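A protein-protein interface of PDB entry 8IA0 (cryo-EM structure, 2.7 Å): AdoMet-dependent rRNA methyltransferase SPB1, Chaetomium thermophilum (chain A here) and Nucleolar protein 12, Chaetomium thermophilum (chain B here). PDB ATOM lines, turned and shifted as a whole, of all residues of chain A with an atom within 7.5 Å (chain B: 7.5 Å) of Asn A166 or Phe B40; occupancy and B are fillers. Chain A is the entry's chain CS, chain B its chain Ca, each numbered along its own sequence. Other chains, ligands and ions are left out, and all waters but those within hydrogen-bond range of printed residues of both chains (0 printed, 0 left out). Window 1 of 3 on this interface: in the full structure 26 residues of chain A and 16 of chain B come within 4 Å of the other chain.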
ATOM      1  N   VAL A 159       7.960  14.474  27.373  1.00  0.00           N
ATOM      2  CA  VAL A 159       6.505  14.431  27.386  1.00  0.00           C
ATOM      3  C   VAL A 159       6.028  14.554  28.823  1.00  0.00           C
ATOM      4  O   VAL A 159       6.413  13.751  29.680  1.00  0.00           O
ATOM      5  CB  VAL A 159       5.970  13.134  26.750  1.00  0.00           C
ATOM      6  CG1 VAL A 159       4.469  13.034  26.935  1.00  0.00           C
ATOM      7  CG2 VAL A 159       6.338  13.079  25.281  1.00  0.00           C
ATOM      8  N   PHE A 160       5.199  15.559  29.090  1.00  0.00           N
ATOM      9  CA  PHE A 160       4.553  15.669  30.388  1.00  0.00           C
ATOM     10  C   PHE A 160       3.544  14.541  30.540  1.00  0.00           C
ATOM     11  O   PHE A 160       2.795  14.238  29.607  1.00  0.00           O
ATOM     12  CB  PHE A 160       3.861  17.022  30.539  1.00  0.00           C
ATOM     13  CG  PHE A 160       4.789  18.148  30.893  1.00  0.00           C
ATOM     14  CD1 PHE A 160       6.156  17.945  30.966  1.00  0.00           C
ATOM     15  CD2 PHE A 160       4.291  19.413  31.156  1.00  0.00           C
ATOM     16  CE1 PHE A 160       7.007  18.982  31.293  1.00  0.00           C
ATOM     17  CE2 PHE A 160       5.138  20.452  31.484  1.00  0.00           C
ATOM     18  CZ  PHE A 160       6.497  20.236  31.551  1.00  0.00           C
ATOM     19  N   ARG A 161       3.524  13.918  31.713  1.00  0.00           N
ATOM     20  CA  ARG A 161       2.611  12.809  31.947  1.00  0.00           C
ATOM     21  C   ARG A 161       1.204  13.343  32.181  1.00  0.00           C
ATOM     22  O   ARG A 161       0.980  14.152  33.088  1.00  0.00           O
ATOM     23  CB  ARG A 161       3.082  11.977  33.136  1.00  0.00           C
ATOM     24  CG  ARG A 161       4.225  11.030  32.807  1.00  0.00           C
ATOM     25  CD  ARG A 161       4.700  10.296  34.045  1.00  0.00           C
ATOM     26  NE  ARG A 161       5.524  11.144  34.895  1.00  0.00           N
ATOM     27  CZ  ARG A 161       6.382  10.693  35.799  1.00  0.00           C
ATOM     28  NH1 ARG A 161       6.560   9.397  35.994  1.00  0.00           N
ATOM     29  NH2 ARG A 161       7.072  11.563  36.530  1.00  0.00           N
ATOM     30  N   SER A 162       0.262  12.898  31.360  1.00  0.00           N
ATOM     31  CA  SER A 162      -1.117  13.360  31.425  1.00  0.00           C
ATOM     32  C   SER A 162      -1.994  12.300  30.765  1.00  0.00           C
ATOM     33  O   SER A 162      -1.542  11.175  30.523  1.00  0.00           O
ATOM     34  CB  SER A 162      -1.251  14.742  30.766  1.00  0.00           C
ATOM     35  OG  SER A 162      -0.752  14.724  29.440  1.00  0.00           O
ATOM     36  N   LYS A 163      -3.243  12.654  30.472  1.00  0.00           N
ATOM     37  CA  LYS A 163      -4.133  11.734  29.778  1.00  0.00           C
ATOM     38  C   LYS A 163      -3.856  11.664  28.283  1.00  0.00           C
ATOM     39  O   LYS A 163      -4.410  10.789  27.608  1.00  0.00           O
ATOM     40  CB  LYS A 163      -5.592  12.121  30.022  1.00  0.00           C
ATOM     41  CG  LYS A 163      -5.999  13.450  29.422  1.00  0.00           C
ATOM     42  CD  LYS A 163      -7.449  13.761  29.750  1.00  0.00           C
ATOM     43  CE  LYS A 163      -7.889  15.065  29.117  1.00  0.00           C
ATOM     44  NZ  LYS A 163      -9.308  15.381  29.441  1.00  0.00           N
ATOM     45  N   ASP A 164      -3.020  12.555  27.752  1.00  0.00           N
ATOM     46  CA  ASP A 164      -2.563  12.467  26.372  1.00  0.00           C
ATOM     47  C   ASP A 164      -1.242  11.725  26.239  1.00  0.00           C
ATOM     48  O   ASP A 164      -0.750  11.565  25.118  1.00  0.00           O
ATOM     49  CB  ASP A 164      -2.418  13.869  25.768  1.00  0.00           C
ATOM     50  CG  ASP A 164      -3.467  14.835  26.279  1.00  0.00           C
ATOM     51  OD1 ASP A 164      -4.663  14.477  26.269  1.00  0.00           O
ATOM     52  OD2 ASP A 164      -3.094  15.953  26.692  1.00  0.00           O
ATOM     53  N   TYR A 165      -0.660  11.278  27.353  1.00  0.00           N
ATOM     54  CA  TYR A 165       0.611  10.567  27.302  1.00  0.00           C
ATOM     55  C   TYR A 165       0.474   9.237  26.572  1.00  0.00           C
ATOM     56  O   TYR A 165       1.350   8.859  25.785  1.00  0.00           O
ATOM     57  CB  TYR A 165       1.141  10.360  28.721  1.00  0.00           C
ATOM     58  CG  TYR A 165       2.313   9.411  28.825  1.00  0.00           C
ATOM     59  CD1 TYR A 165       3.565   9.770  28.352  1.00  0.00           C
ATOM     60  CD2 TYR A 165       2.166   8.164  29.411  1.00  0.00           C
ATOM     61  CE1 TYR A 165       4.637   8.909  28.451  1.00  0.00           C
ATOM     62  CE2 TYR A 165       3.231   7.296  29.514  1.00  0.00           C
ATOM     63  CZ  TYR A 165       4.464   7.673  29.032  1.00  0.00           C
ATOM     64  OH  TYR A 165       5.529   6.808  29.135  1.00  0.00           O
ATOM     65  N   ASN A 166      -0.618   8.510  26.820  1.00  0.00           N
ATOM     66  CA  ASN A 166      -0.814   7.228  26.155  1.00  0.00           C
ATOM     67  C   ASN A 166      -1.159   7.402  24.683  1.00  0.00           C
ATOM     68  O   ASN A 166      -0.806   6.551  23.861  1.00  0.00           O
ATOM     69  CB  ASN A 166      -1.909   6.432  26.859  1.00  0.00           C
ATOM     70  CG  ASN A 166      -1.417   5.754  28.118  1.00  0.00           C
ATOM     71  OD1 ASN A 166      -1.938   5.990  29.208  1.00  0.00           O
ATOM     72  ND2 ASN A 166      -0.403   4.909  27.978  1.00  0.00           N
ATOM     73  N   LYS A 167      -1.851   8.487  24.334  1.00  0.00           N
ATOM     74  CA  LYS A 167      -2.237   8.697  22.944  1.00  0.00           C
ATOM     75  C   LYS A 167      -1.027   9.023  22.078  1.00  0.00           C
ATOM     76  O   LYS A 167      -0.980   8.643  20.902  1.00  0.00           O
ATOM     77  CB  LYS A 167      -3.285   9.802  22.855  1.00  0.00           C
ATOM     78  CG  LYS A 167      -4.511   9.541  23.711  1.00  0.00           C
ATOM     79  CD  LYS A 167      -5.541  10.640  23.559  1.00  0.00           C
ATOM     80  CE  LYS A 167      -6.756  10.366  24.424  1.00  0.00           C
ATOM     81  NZ  LYS A 167      -7.803  11.407  24.251  1.00  0.00           N
ATOM     82  N   LEU A 168      -0.043   9.729  22.636  1.00  0.00           N
ATOM     83  CA  LEU A 168       1.181   9.993  21.889  1.00  0.00           C
ATOM     84  C   LEU A 168       2.052   8.748  21.776  1.00  0.00           C
ATOM     85  O   LEU A 168       2.730   8.560  20.762  1.00  0.00           O
ATOM     86  CB  LEU A 168       1.967  11.128  22.540  1.00  0.00           C
ATOM     87  CG  LEU A 168       3.058  11.740  21.662  1.00  0.00           C
ATOM     88  CD1 LEU A 168       2.473  12.812  20.763  1.00  0.00           C
ATOM     89  CD2 LEU A 168       4.183  12.302  22.507  1.00  0.00           C
ATOM     90  N   LEU A 169       2.053   7.896  22.804  1.00  0.00           N
ATOM     91  CA  LEU A 169       2.855   6.678  22.757  1.00  0.00           C
ATOM     92  C   LEU A 169       2.381   5.745  21.650  1.00  0.00           C
ATOM     93  O   LEU A 169       3.182   5.011  21.061  1.00  0.00           O
ATOM     94  CB  LEU A 169       2.813   5.967  24.109  1.00  0.00           C
ATOM     95  CG  LEU A 169       4.100   6.007  24.931  1.00  0.00           C
ATOM     96  CD1 LEU A 169       4.506   7.443  25.212  1.00  0.00           C
ATOM     97  CD2 LEU A 169       3.930   5.233  26.225  1.00  0.00           C
ATOM     98  N   TRP A 170       1.079   5.752  21.363  1.00  0.00           N
ATOM     99  CA  TRP A 170       0.555   4.919  20.286  1.00  0.00           C
ATOM    100  C   TRP A 170       1.082   5.374  18.932  1.00  0.00           C
ATOM    101  O   TRP A 170       1.152   4.581  17.986  1.00  0.00           O
ATOM    102  CB  TRP A 170      -0.973   4.942  20.310  1.00  0.00           C
ATOM    103  CG  TRP A 170      -1.617   4.151  19.216  1.00  0.00           C
ATOM    104  CD1 TRP A 170      -1.878   2.815  19.218  1.00  0.00           C
ATOM    105  CD2 TRP A 170      -2.102   4.653  17.966  1.00  0.00           C
ATOM    106  NE1 TRP A 170      -2.486   2.451  18.043  1.00  0.00           N
ATOM    107  CE2 TRP A 170      -2.635   3.562  17.257  1.00  0.00           C
ATOM    108  CE3 TRP A 170      -2.132   5.919  17.376  1.00  0.00           C
ATOM    109  CZ2 TRP A 170      -3.191   3.697  15.989  1.00  0.00           C
ATOM    110  CZ3 TRP A 170      -2.684   6.050  16.118  1.00  0.00           C
ATOM    111  CH2 TRP A 170      -3.206   4.947  15.439  1.00  0.00           C
ATOM    112  N   VAL A 171       1.462   6.648  18.819  1.00  0.00           N
ATOM    113  CA  VAL A 171       1.969   7.159  17.548  1.00  0.00           C
ATOM    114  C   VAL A 171       3.353   6.589  17.254  1.00  0.00           C
ATOM    115  O   VAL A 171       3.619   6.107  16.147  1.00  0.00           O
ATOM    116  CB  VAL A 171       1.972   8.698  17.552  1.00  0.00           C
ATOM    117  CG1 VAL A 171       3.057   9.237  16.635  1.00  0.00           C
ATOM    118  CG2 VAL A 171       0.614   9.223  17.129  1.00  0.00           C
ATOM    119  N   ASN A 173       4.479   3.902  18.429  1.00  0.00           N
ATOM    120  CA  ASN A 173       4.301   2.465  18.255  1.00  0.00           C
ATOM    121  C   ASN A 173       4.025   2.117  16.798  1.00  0.00           C
ATOM    122  O   ASN A 173       4.605   1.170  16.254  1.00  0.00           O
ATOM    123  CB  ASN A 173       3.168   1.968  19.150  1.00  0.00           C
ATOM    124  CG  ASN A 173       3.670   1.400  20.456  1.00  0.00           C
ATOM    125  OD1 ASN A 173       4.870   1.390  20.716  1.00  0.00           O
ATOM    126  ND2 ASN A 173       2.753   0.923  21.290  1.00  0.00           N
ATOM    127  N   ILE A 217      -5.247  12.390  16.706  1.00  0.00           N
ATOM    128  CA  ILE A 217      -4.578  11.629  17.762  1.00  0.00           C
ATOM    129  C   ILE A 217      -5.146  11.963  19.130  1.00  0.00           C
ATOM    130  O   ILE A 217      -5.394  11.074  19.949  1.00  0.00           O
ATOM    131  CB  ILE A 217      -3.048  11.857  17.725  1.00  0.00           C
ATOM    132  CG1 ILE A 217      -2.489  11.881  16.296  1.00  0.00           C
ATOM    133  CG2 ILE A 217      -2.337  10.804  18.561  1.00  0.00           C
ATOM    134  CD1 ILE A 217      -3.040  10.800  15.372  1.00  0.00           C
ATOM    135  N   PHE A 218      -5.373  13.244  19.396  1.00  0.00           N
ATOM    136  CA  PHE A 218      -5.829  13.697  20.699  1.00  0.00           C
ATOM    137  C   PHE A 218      -7.346  13.721  20.803  1.00  0.00           C
ATOM    138  O   PHE A 218      -7.880  14.174  21.820  1.00  0.00           O
ATOM    139  CB  PHE A 218      -5.251  15.081  20.999  1.00  0.00           C
ATOM    140  CG  PHE A 218      -3.774  15.068  21.287  1.00  0.00           C
ATOM    141  CD1 PHE A 218      -3.069  13.878  21.303  1.00  0.00           C
ATOM    142  CD2 PHE A 218      -3.091  16.245  21.524  1.00  0.00           C
ATOM    143  CE1 PHE A 218      -1.717  13.862  21.560  1.00  0.00           C
ATOM    144  CE2 PHE A 218      -1.736  16.234  21.782  1.00  0.00           C
ATOM    145  CZ  PHE A 218      -1.050  15.038  21.798  1.00  0.00           C
ATOM    146  N   ARG B  33      -6.269   1.449  17.586  1.00  0.00           N
ATOM    147  CA  ARG B  33      -6.059   2.514  18.561  1.00  0.00           C
ATOM    148  C   ARG B  33      -7.007   2.371  19.744  1.00  0.00           C
ATOM    149  O   ARG B  33      -6.605   2.569  20.897  1.00  0.00           O
ATOM    150  CB  ARG B  33      -6.232   3.875  17.892  1.00  0.00           C
ATOM    151  CG  ARG B  33      -6.122   5.051  18.841  1.00  0.00           C
ATOM    152  CD  ARG B  33      -6.052   6.358  18.079  1.00  0.00           C
ATOM    153  NE  ARG B  33      -6.100   7.510  18.970  1.00  0.00           N
ATOM    154  CZ  ARG B  33      -7.217   8.112  19.348  1.00  0.00           C
ATOM    155  NH1 ARG B  33      -8.401   7.694  18.932  1.00  0.00           N
ATOM    156  NH2 ARG B  33      -7.146   9.160  20.162  1.00  0.00           N
ATOM    157  N   GLU B  35      -8.353  -0.458  20.768  1.00  0.00           N
ATOM    158  CA  GLU B  35      -7.903  -1.632  21.507  1.00  0.00           C
ATOM    159  C   GLU B  35      -6.682  -1.311  22.360  1.00  0.00           C
ATOM    160  O   GLU B  35      -6.594  -1.742  23.515  1.00  0.00           O
ATOM    161  CB  GLU B  35      -7.603  -2.773  20.535  1.00  0.00           C
ATOM    162  CG  GLU B  35      -6.502  -3.728  20.980  1.00  0.00           C
ATOM    163  CD  GLU B  35      -6.875  -4.519  22.218  1.00  0.00           C
ATOM    164  OE1 GLU B  35      -7.997  -5.068  22.260  1.00  0.00           O
ATOM    165  OE2 GLU B  35      -6.048  -4.594  23.150  1.00  0.00           O
ATOM    166  N   TYR B  36      -5.731  -0.553  21.810  1.00  0.00           N
ATOM    167  CA  TYR B  36      -4.531  -0.219  22.569  1.00  0.00           C
ATOM    168  C   TYR B  36      -4.855   0.676  23.759  1.00  0.00           C
ATOM    169  O   TYR B  36      -4.355   0.449  24.867  1.00  0.00           O
ATOM    170  CB  TYR B  36      -3.503   0.459  21.664  1.00  0.00           C
ATOM    171  CG  TYR B  36      -2.325   1.027  22.422  1.00  0.00           C
ATOM    172  CD1 TYR B  36      -1.354   0.193  22.953  1.00  0.00           C
ATOM    173  CD2 TYR B  36      -2.192   2.394  22.618  1.00  0.00           C
ATOM    174  CE1 TYR B  36      -0.279   0.702  23.652  1.00  0.00           C
ATOM    175  CE2 TYR B  36      -1.121   2.913  23.316  1.00  0.00           C
ATOM    176  CZ  TYR B  36      -0.168   2.062  23.831  1.00  0.00           C
ATOM    177  OH  TYR B  36       0.902   2.574  24.526  1.00  0.00           O
ATOM    178  N   LEU B  37      -5.687   1.698  23.551  1.00  0.00           N
ATOM    179  CA  LEU B  37      -5.967   2.658  24.612  1.00  0.00           C
ATOM    180  C   LEU B  37      -6.894   2.097  25.680  1.00  0.00           C
ATOM    181  O   LEU B  37      -6.651   2.308  26.873  1.00  0.00           O
ATOM    182  CB  LEU B  37      -6.565   3.933  24.019  1.00  0.00           C
ATOM    183  CG  LEU B  37      -5.574   4.818  23.264  1.00  0.00           C
ATOM    184  CD1 LEU B  37      -6.295   5.945  22.547  1.00  0.00           C
ATOM    185  CD2 LEU B  37      -4.527   5.366  24.215  1.00  0.00           C
ATOM    186  N   THR B  38      -7.951   1.387  25.287  1.00  0.00           N
ATOM    187  CA  THR B  38      -8.894   0.860  26.264  1.00  0.00           C
ATOM    188  C   THR B  38      -8.324  -0.301  27.059  1.00  0.00           C
ATOM    189  O   THR B  38      -8.626  -0.435  28.249  1.00  0.00           O
ATOM    190  CB  THR B  38     -10.186   0.405  25.579  1.00  0.00           C
ATOM    191  OG1 THR B  38      -9.878  -0.160  24.302  1.00  0.00           O
ATOM    192  CG2 THR B  38     -11.131   1.581  25.391  1.00  0.00           C
ATOM    193  N   GLY B  39      -7.507  -1.140  26.433  1.00  0.00           N
ATOM    194  CA  GLY B  39      -6.959  -2.291  27.118  1.00  0.00           C
ATOM    195  C   GLY B  39      -5.599  -2.052  27.735  1.00  0.00           C
ATOM    196  O   GLY B  39      -4.574  -2.132  27.055  1.00  0.00           O
ATOM    197  N   PHE B  40      -5.583  -1.756  29.030  1.00  0.00           N
ATOM    198  CA  PHE B  40      -4.360  -1.710  29.820  1.00  0.00           C
ATOM    199  C   PHE B  40      -4.444  -2.616  31.033  1.00  0.00           C
ATOM    200  O   PHE B  40      -3.451  -3.256  31.398  1.00  0.00           O
ATOM    201  CB  PHE B  40      -4.056  -0.270  30.262  1.00  0.00           C
ATOM    202  CG  PHE B  40      -3.127   0.465  29.342  1.00  0.00           C
ATOM    203  CD1 PHE B  40      -3.596   1.034  28.173  1.00  0.00           C
ATOM    204  CD2 PHE B  40      -1.785   0.591  29.652  1.00  0.00           C
ATOM    205  CE1 PHE B  40      -2.743   1.712  27.328  1.00  0.00           C
ATOM    206  CE2 PHE B  40      -0.928   1.268  28.812  1.00  0.00           C
ATOM    207  CZ  PHE B  40      -1.408   1.828  27.648  1.00  0.00           C
ATOM    208  N   ARG B  41      -5.610  -2.683  31.676  1.00  0.00           N
ATOM    209  CA  ARG B  41      -5.802  -3.638  32.760  1.00  0.00           C
ATOM    210  C   ARG B  41      -5.857  -5.063  32.225  1.00  0.00           C
ATOM    211  O   ARG B  41      -5.360  -5.995  32.868  1.00  0.00           O
ATOM    212  CB  ARG B  41      -7.076  -3.299  33.535  1.00  0.00           C
ATOM    213  CG  ARG B  41      -7.337  -4.191  34.737  1.00  0.00           C
ATOM    214  CD  ARG B  41      -8.389  -3.583  35.652  1.00  0.00           C
ATOM    215  NE  ARG B  41      -8.991  -4.575  36.535  1.00  0.00           N
ATOM    216  CZ  ARG B  41      -8.456  -4.985  37.676  1.00  0.00           C
ATOM    217  NH1 ARG B  41      -7.300  -4.508  38.108  1.00  0.00           N
ATOM    218  NH2 ARG B  41      -9.097  -5.895  38.404  1.00  0.00           N
ATOM    219  N   LYS B  42      -6.458  -5.254  31.047  1.00  0.00           N
ATOM    220  CA  LYS B  42      -6.565  -6.596  30.485  1.00  0.00           C
ATOM    221  C   LYS B  42      -5.201  -7.143  30.077  1.00  0.00           C
ATOM    222  O   LYS B  42      -4.925  -8.332  30.271  1.00  0.00           O
ATOM    223  CB  LYS B  42      -7.535  -6.605  29.302  1.00  0.00           C
ATOM    224  CG  LYS B  42      -7.112  -5.760  28.116  1.00  0.00           C
ATOM    225  CD  LYS B  42      -8.150  -5.813  27.008  1.00  0.00           C
ATOM    226  CE  LYS B  42      -8.256  -7.210  26.418  1.00  0.00           C
ATOM    227  NZ  LYS B  42      -9.266  -7.280  25.326  1.00  0.00           N
ATOM    228  N   ARG B  43      -4.335  -6.300  29.508  1.00  0.00           N
ATOM    229  CA  ARG B  43      -2.994  -6.766  29.167  1.00  0.00           C
ATOM    230  C   ARG B  43      -2.176  -7.035  30.421  1.00  0.00           C
ATOM    231  O   ARG B  43      -1.382  -7.982  30.459  1.00  0.00           O
ATOM    232  CB  ARG B  43      -2.278  -5.758  28.271  1.00  0.00           C
ATOM    233  CG  ARG B  43      -2.947  -5.515  26.934  1.00  0.00           C
ATOM    234  CD  ARG B  43      -2.020  -4.768  25.991  1.00  0.00           C
ATOM    235  NE  ARG B  43      -2.522  -3.444  25.650  1.00  0.00           N
ATOM    236  CZ  ARG B  43      -1.870  -2.315  25.895  1.00  0.00           C
ATOM    237  NH1 ARG B  43      -0.672  -2.317  26.455  1.00  0.00           N
ATOM    238  NH2 ARG B  43      -2.436  -1.157  25.572  1.00  0.00           N
ATOM    239  N   LYS B  44      -2.348  -6.207  31.452  1.00  0.00           N
ATOM    240  CA  LYS B  44      -1.673  -6.465  32.718  1.00  0.00           C
ATOM    241  C   LYS B  44      -2.147  -7.775  33.332  1.00  0.00           C
ATOM    242  O   LYS B  44      -1.329  -8.589  33.774  1.00  0.00           O
ATOM    243  CB  LYS B  44      -1.908  -5.304  33.684  1.00  0.00           C
ATOM    244  CG  LYS B  44      -1.321  -5.519  35.068  1.00  0.00           C
ATOM    245  CD  LYS B  44       0.189  -5.650  35.017  1.00  0.00           C
ATOM    246  CE  LYS B  44       0.816  -5.236  36.336  1.00  0.00           C
ATOM    247  NZ  LYS B  44       0.100  -4.084  36.947  1.00  0.00           N
ATOM    248  N   GLN B  45      -3.462  -8.004  33.347  1.00  0.00           N
ATOM    249  CA  GLN B  45      -3.994  -9.236  33.922  1.00  0.00           C
ATOM    250  C   GLN B  45      -3.522 -10.458  33.145  1.00  0.00           C
ATOM    251  O   GLN B  45      -3.297 -11.525  33.727  1.00  0.00           O
ATOM    252  CB  GLN B  45      -5.520  -9.180  33.963  1.00  0.00           C
ATOM    253  CG  GLN B  45      -6.077  -8.327  35.088  1.00  0.00           C
ATOM    254  CD  GLN B  45      -5.583  -8.769  36.451  1.00  0.00           C
ATOM    255  OE1 GLN B  45      -4.938  -8.003  37.169  1.00  0.00           O
ATOM    256  NE2 GLN B  45      -5.882 -10.010  36.815  1.00  0.00           N
ATOM    257  N   ALA B  46      -3.377 -10.325  31.825  1.00  0.00           N
ATOM    258  CA  ALA B  46      -2.857 -11.427  31.025  1.00  0.00           C
ATOM    259  C   ALA B  46      -1.426 -11.766  31.419  1.00  0.00           C
ATOM    260  O   ALA B  46      -1.051 -12.944  31.475  1.00  0.00           O
ATOM    261  CB  ALA B  46      -2.936 -11.082  29.538  1.00  0.00           C
ATOM    262  N   ARG B  47      -0.609 -10.748  31.691  1.00  0.00           N
ATOM    263  CA  ARG B  47       0.784 -10.992  32.055  1.00  0.00           C
ATOM    264  C   ARG B  47       0.896 -11.667  33.416  1.00  0.00           C
ATOM    265  O   ARG B  47       1.724 -12.565  33.602  1.00  0.00           O
ATOM    266  CB  ARG B  47       1.567  -9.681  32.030  1.00  0.00           C
ATOM    267  CG  ARG B  47       1.756  -9.114  30.633  1.00  0.00           C
ATOM    268  CD  ARG B  47       2.917  -8.140  30.577  1.00  0.00           C
ATOM    269  NE  ARG B  47       2.735  -7.026  31.499  1.00  0.00           N
ATOM    270  CZ  ARG B  47       2.161  -5.876  31.177  1.00  0.00           C
ATOM    271  NH1 ARG B  47       1.701  -5.651  29.957  1.00  0.00           N
ATOM    272  NH2 ARG B  47       2.046  -4.927  32.101  1.00  0.00           N
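Of the 14 printed residues of chain B, 4 touch a printed residue of chain A. Hydrophobic or aromatic side chains of chain B within 4 Å of the printed part of chain A: Tyr B36, Leu B37 and Phe B40. Hydrophobic or aromatic side chains of chain A within 4 Å of the printed part of chain B: Leu A169 and Trp A170. Among the printed residues, no Asp or Glu carboxylate lies within 4 Å of a Lys or Arg side-chain nitrogen of the other chain.
Among the printed residues, merely in contact across the chains: Asn A166 with Phe B40 (3.3 Å), Trp A170 with Tyr B36 (3.4 Å), Trp A170 with Arg B33 (3.6 Å), Asn A166 with Tyr B36 (3.7 Å), Asn A173 with Tyr B36 (3.8 Å), Asn A166 with Leu B37 (3.9 Å) and Leu A169 with Tyr B36 (3.9 Å).
Asn A166 touches just these residues of chain B: Tyr B36, Leu B37 and Phe B40. Phe B40 touches one residue of chain A. Of the printed residues of chain B, Leu A169 touches Tyr B36. Printed residues of chain A within 4 Å of Tyr B36: Asn A166, Leu A169, Trp A170 and Asn A173. Of the printed residues of chain A, Arg B33 touches Trp A170 and Ile A217. Of the printed residues of chain B, Trp A170 touches Arg B33 and Tyr B36. Ala B46 touches none of the printed residues of chain A. The nearest residue of chain A that does not touch Phe B40 is Leu A169 (6.5 Å). The nearest printed residue of chain A that does not touch Arg B33 is Lys A167 (4.04 Å).
The guanidinium group of Arg B33 lies within hydrogen-bond range of the backbone carbonyl oxygen of Ile A217, at 2.6 Å.
The guanidinium group of Arg B43 lies within hydrogen-bond range of the backbone carbonyl oxygen of Tyr B36.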
